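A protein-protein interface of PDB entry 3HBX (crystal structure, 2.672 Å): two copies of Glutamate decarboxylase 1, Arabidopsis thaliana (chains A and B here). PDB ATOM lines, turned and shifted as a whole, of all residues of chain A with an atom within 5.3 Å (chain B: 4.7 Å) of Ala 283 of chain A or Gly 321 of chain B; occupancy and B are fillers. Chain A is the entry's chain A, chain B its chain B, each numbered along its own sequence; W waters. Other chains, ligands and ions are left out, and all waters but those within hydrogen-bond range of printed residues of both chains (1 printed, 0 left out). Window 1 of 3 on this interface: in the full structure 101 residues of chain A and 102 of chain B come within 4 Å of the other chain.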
ATOM      1  N   VAL A  64       6.902  12.984  -7.790  1.00  0.00           N
ATOM      2  CA  VAL A  64       6.189  12.184  -6.797  1.00  0.00           C
ATOM      3  C   VAL A  64       4.838  11.674  -7.296  1.00  0.00           C
ATOM      4  O   VAL A  64       4.050  12.422  -7.870  1.00  0.00           O
ATOM      5  CB  VAL A  64       6.004  12.957  -5.474  1.00  0.00           C
ATOM      6  CG1 VAL A  64       5.112  12.179  -4.523  1.00  0.00           C
ATOM      7  CG2 VAL A  64       7.355  13.230  -4.833  1.00  0.00           C
ATOM      8  N   THR A  65       4.587  10.389  -7.065  1.00  0.00           N
ATOM      9  CA  THR A  65       3.353   9.738  -7.496  1.00  0.00           C
ATOM     10  C   THR A  65       2.105  10.424  -6.942  1.00  0.00           C
ATOM     11  O   THR A  65       2.046  10.774  -5.764  1.00  0.00           O
ATOM     12  CB  THR A  65       3.345   8.255  -7.089  1.00  0.00           C
ATOM     13  OG1 THR A  65       4.367   7.562  -7.815  1.00  0.00           O
ATOM     14  CG2 THR A  65       1.998   7.621  -7.388  1.00  0.00           C
ATOM     15  N   HIS A 276       8.204   6.874  -3.346  1.00  0.00           N
ATOM     16  CA  HIS A 276       7.116   7.773  -3.710  1.00  0.00           C
ATOM     17  C   HIS A 276       7.369   8.516  -5.015  1.00  0.00           C
ATOM     18  O   HIS A 276       6.575   9.368  -5.410  1.00  0.00           O
ATOM     19  CB  HIS A 276       6.808   8.765  -2.586  1.00  0.00           C
ATOM     20  CG  HIS A 276       7.978   9.598  -2.169  1.00  0.00           C
ATOM     21  ND1 HIS A 276       8.325   9.787  -0.850  1.00  0.00           N
ATOM     22  CD2 HIS A 276       8.887  10.287  -2.901  1.00  0.00           C
ATOM     23  CE1 HIS A 276       9.392  10.563  -0.785  1.00  0.00           C
ATOM     24  NE2 HIS A 276       9.754  10.880  -2.014  1.00  0.00           N
ATOM     25  N   VAL A 281       4.280   4.982  -5.168  1.00  0.00           N
ATOM     26  CA  VAL A 281       3.589   5.128  -3.893  1.00  0.00           C
ATOM     27  C   VAL A 281       3.365   6.606  -3.603  1.00  0.00           C
ATOM     28  O   VAL A 281       4.108   7.455  -4.093  1.00  0.00           O
ATOM     29  CB  VAL A 281       4.401   4.501  -2.741  1.00  0.00           C
ATOM     30  CG1 VAL A 281       3.653   4.629  -1.424  1.00  0.00           C
ATOM     31  CG2 VAL A 281       4.710   3.045  -3.041  1.00  0.00           C
ATOM     32  N   TYR A 282       2.333   6.919  -2.823  1.00  0.00           N
ATOM     33  CA  TYR A 282       2.108   8.294  -2.391  1.00  0.00           C
ATOM     34  C   TYR A 282       3.307   8.781  -1.579  1.00  0.00           C
ATOM     35  O   TYR A 282       4.067   7.978  -1.036  1.00  0.00           O
ATOM     36  CB  TYR A 282       0.834   8.414  -1.550  1.00  0.00           C
ATOM     37  CG  TYR A 282      -0.456   8.172  -2.307  1.00  0.00           C
ATOM     38  CD1 TYR A 282      -0.791   8.933  -3.423  1.00  0.00           C
ATOM     39  CD2 TYR A 282      -1.353   7.199  -1.888  1.00  0.00           C
ATOM     40  CE1 TYR A 282      -1.975   8.717  -4.107  1.00  0.00           C
ATOM     41  CE2 TYR A 282      -2.536   6.977  -2.562  1.00  0.00           C
ATOM     42  CZ  TYR A 282      -2.843   7.737  -3.669  1.00  0.00           C
ATOM     43  OH  TYR A 282      -4.026   7.508  -4.335  1.00  0.00           O
ATOM     44  N   ALA A 283       3.466  10.097  -1.491  1.00  0.00           N
ATOM     45  CA  ALA A 283       4.595  10.688  -0.780  1.00  0.00           C
ATOM     46  C   ALA A 283       4.738  10.145   0.636  1.00  0.00           C
ATOM     47  O   ALA A 283       3.751  10.007   1.358  1.00  0.00           O
ATOM     48  CB  ALA A 283       4.468  12.204  -0.755  1.00  0.00           C
ATOM     49  N   GLY A 284       5.972   9.838   1.030  1.00  0.00           N
ATOM     50  CA  GLY A 284       6.256   9.415   2.389  1.00  0.00           C
ATOM     51  C   GLY A 284       7.021   8.110   2.517  1.00  0.00           C
ATOM     52  O   GLY A 284       6.966   7.456   3.560  1.00  0.00           O
ATOM     53  N   ILE A 285       7.742   7.726   1.467  1.00  0.00           N
ATOM     54  CA  ILE A 285       8.519   6.487   1.509  1.00  0.00           C
ATOM     55  C   ILE A 285       9.788   6.528   0.651  1.00  0.00           C
ATOM     56  O   ILE A 285       9.753   6.874  -0.530  1.00  0.00           O
ATOM     57  CB  ILE A 285       7.664   5.268   1.105  1.00  0.00           C
ATOM     58  CG1 ILE A 285       8.475   3.978   1.232  1.00  0.00           C
ATOM     59  CG2 ILE A 285       7.119   5.436  -0.304  1.00  0.00           C
ATOM     60  CD1 ILE A 285       8.901   3.665   2.647  1.00  0.00           C
ATOM     61  N   GLN A 324       2.702   3.979   4.047  1.00  0.00           N
ATOM     62  CA  GLN A 324       3.510   4.002   2.830  1.00  0.00           C
ATOM     63  C   GLN A 324       4.346   2.735   2.686  1.00  0.00           C
ATOM     64  O   GLN A 324       4.544   2.238   1.580  1.00  0.00           O
ATOM     65  CB  GLN A 324       4.403   5.242   2.778  1.00  0.00           C
ATOM     66  CG  GLN A 324       3.652   6.548   2.575  1.00  0.00           C
ATOM     67  CD  GLN A 324       3.307   7.226   3.883  1.00  0.00           C
ATOM     68  OE1 GLN A 324       3.484   6.652   4.958  1.00  0.00           O
ATOM     69  NE2 GLN A 324       2.820   8.459   3.801  1.00  0.00           N
ATOM     70  N   ILE B  80      -3.676  12.699   0.344  1.00  0.00           N
ATOM     71  CA  ILE B  80      -2.565  11.755   0.449  1.00  0.00           C
ATOM     72  C   ILE B  80      -1.646  11.854  -0.761  1.00  0.00           C
ATOM     73  O   ILE B  80      -0.519  11.363  -0.734  1.00  0.00           O
ATOM     74  CB  ILE B  80      -3.027  10.287   0.631  1.00  0.00           C
ATOM     75  CG1 ILE B  80      -4.371  10.047  -0.059  1.00  0.00           C
ATOM     76  CG2 ILE B  80      -3.109   9.929   2.109  1.00  0.00           C
ATOM     77  CD1 ILE B  80      -4.296  10.061  -1.565  1.00  0.00           C
ATOM     78  N   LYS B  82      -0.910  14.900  -2.133  1.00  0.00           N
ATOM     79  CA  LYS B  82      -0.260  16.206  -2.081  1.00  0.00           C
ATOM     80  C   LYS B  82       1.106  16.116  -1.407  1.00  0.00           C
ATOM     81  O   LYS B  82       1.196  15.998  -0.187  1.00  0.00           O
ATOM     82  CB  LYS B  82      -1.124  17.226  -1.333  1.00  0.00           C
ATOM     83  CG  LYS B  82      -2.256  17.840  -2.143  1.00  0.00           C
ATOM     84  CD  LYS B  82      -2.764  19.109  -1.467  1.00  0.00           C
ATOM     85  CE  LYS B  82      -4.183  19.450  -1.889  1.00  0.00           C
ATOM     86  NZ  LYS B  82      -4.273  19.838  -3.322  1.00  0.00           N
ATOM     87  N   ASN B  83       2.168  16.166  -2.204  1.00  0.00           N
ATOM     88  CA  ASN B  83       3.521  16.217  -1.667  1.00  0.00           C
ATOM     89  C   ASN B  83       3.774  17.574  -1.024  1.00  0.00           C
ATOM     90  O   ASN B  83       3.744  18.603  -1.699  1.00  0.00           O
ATOM     91  CB  ASN B  83       4.543  15.961  -2.771  1.00  0.00           C
ATOM     92  CG  ASN B  83       5.968  15.985  -2.262  1.00  0.00           C
ATOM     93  OD1 ASN B  83       6.212  16.156  -1.069  1.00  0.00           O
ATOM     94  ND2 ASN B  83       6.922  15.811  -3.169  1.00  0.00           N
ATOM     95  N   TYR B  84       4.027  17.577   0.280  1.00  0.00           N
ATOM     96  CA  TYR B  84       4.144  18.831   1.019  1.00  0.00           C
ATOM     97  C   TYR B  84       5.204  19.786   0.469  1.00  0.00           C
ATOM     98  O   TYR B  84       5.004  21.000   0.444  1.00  0.00           O
ATOM     99  CB  TYR B  84       4.414  18.589   2.507  1.00  0.00           C
ATOM    100  CG  TYR B  84       4.610  19.889   3.247  1.00  0.00           C
ATOM    101  CD1 TYR B  84       3.519  20.639   3.667  1.00  0.00           C
ATOM    102  CD2 TYR B  84       5.883  20.390   3.486  1.00  0.00           C
ATOM    103  CE1 TYR B  84       3.688  21.840   4.320  1.00  0.00           C
ATOM    104  CE2 TYR B  84       6.064  21.593   4.141  1.00  0.00           C
ATOM    105  CZ  TYR B  84       4.962  22.313   4.556  1.00  0.00           C
ATOM    106  OH  TYR B  84       5.129  23.510   5.208  1.00  0.00           O
ATOM    107  N   LYS B 320       7.314  14.516   1.392  1.00  0.00           N
ATOM    108  CA  LYS B 320       6.573  13.852   2.454  1.00  0.00           C
ATOM    109  C   LYS B 320       5.104  14.215   2.344  1.00  0.00           C
ATOM    110  O   LYS B 320       4.752  15.215   1.715  1.00  0.00           O
ATOM    111  CB  LYS B 320       7.105  14.263   3.828  1.00  0.00           C
ATOM    112  CG  LYS B 320       6.934  15.739   4.145  1.00  0.00           C
ATOM    113  CD  LYS B 320       7.049  16.000   5.639  1.00  0.00           C
ATOM    114  CE  LYS B 320       6.785  17.463   5.966  1.00  0.00           C
ATOM    115  NZ  LYS B 320       6.621  17.691   7.428  1.00  0.00           N
ATOM    116  N   GLY B 321       4.249  13.401   2.950  1.00  0.00           N
ATOM    117  CA  GLY B 321       2.822  13.662   2.939  1.00  0.00           C
ATOM    118  C   GLY B 321       2.493  14.969   3.629  1.00  0.00           C
ATOM    119  O   GLY B 321       3.184  15.378   4.563  1.00  0.00           O
ATOM    120  N   SER B 322       1.437  15.632   3.167  1.00  0.00           N
ATOM    121  CA  SER B 322       0.999  16.883   3.773  1.00  0.00           C
ATOM    122  C   SER B 322      -0.311  16.688   4.523  1.00  0.00           C
ATOM    123  O   SER B 322      -0.889  17.641   5.044  1.00  0.00           O
ATOM    124  CB  SER B 322       0.838  17.966   2.707  1.00  0.00           C
ATOM    125  OG  SER B 322      -0.116  17.574   1.737  1.00  0.00           O
ATOM    126  N   SER B 323      -0.770  15.442   4.579  1.00  0.00           N
ATOM    127  CA  SER B 323      -2.041  15.118   5.218  1.00  0.00           C
ATOM    128  C   SER B 323      -2.024  15.378   6.722  1.00  0.00           C
ATOM    129  O   SER B 323      -3.004  15.868   7.282  1.00  0.00           O
ATOM    130  CB  SER B 323      -2.437  13.667   4.927  1.00  0.00           C
ATOM    131  OG  SER B 323      -1.327  12.794   5.070  1.00  0.00           O
ATOM    132  N   GLN B 324      -0.912  15.056   7.375  1.00  0.00           N
ATOM    133  CA  GLN B 324      -0.808  15.263   8.816  1.00  0.00           C
ATOM    134  C   GLN B 324      -0.783  16.745   9.173  1.00  0.00           C
ATOM    135  O   GLN B 324      -1.331  17.152  10.196  1.00  0.00           O
ATOM    136  CB  GLN B 324       0.419  14.559   9.397  1.00  0.00           C
ATOM    137  CG  GLN B 324       0.329  13.042   9.389  1.00  0.00           C
ATOM    138  CD  GLN B 324       0.939  12.431   8.144  1.00  0.00           C
ATOM    139  OE1 GLN B 324       1.293  13.140   7.199  1.00  0.00           O
ATOM    140  NE2 GLN B 324       1.075  11.109   8.138  1.00  0.00           N
HETATM  141  O   HOH W   1       2.449   9.067   6.654  1.00  0.00           O
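O of Ala 283 of chain A sits at hydrogen-bond distance from NE2 of Gln 324 of chain A (3.0 Å).
N of Lys 320 of chain B sits at hydrogen-bond distance from OD1 of Asn 83 of chain B (3.2 Å).
N of Tyr 84 of chain B is in hydrogen-bond range of O of Lys 320 of chain B, 2.9 Å away.
Among the printed residues, merely in contact across the chains: Val 64 of chain A with Asn 83 of chain B (3.1 Å), Tyr 282 of chain A with Ile 80 of chain B (3.3 Å), Ala 283 of chain A with Lys 320 of chain B (3.7 Å) and Ala 283 of chain A with Gly 321 of chain B (3.8 Å).
Printed residues of chain B within 4 Å of Val 64 of chain A: Asn 83.
Of the printed residues of chain B, Tyr 282 of chain A touches Ile 80 (3.3 Å).
Ala 283 of chain A touches just these residues of chain B: Lys 320 and Gly 321.
Of the printed residues of chain A, Lys 320 of chain B touches Ala 283.
Of the 9 printed residues of chain B, 4 touch a printed residue of chain A.
Hydrophobic or aromatic side chains of chain B that line the printed part of chain A: Ile 80.
Along chain B the printed residues that touch a printed residue of chain A span positions 80 to 321.
Hydrophobic or aromatic side chains of chain A within 4 Å of the printed part of chain B: Val 64, Tyr 282 and Ala 283.
Among the printed residues, no Asp or Glu carboxylate lies within 4 Å of a Lys or Arg side-chain nitrogen of the other chain.
Position printed for both chains: 324.
Of the 4 pairs that touch across the chains among the printed residues, none has its exchanged pair printed and touching as well.
Water W1 bridges the side-chain amide nitrogen of Gln 324 of chain B (2.9 Å) and the side-chain amide nitrogen of Gln 324 of chain A (2.9 Å).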
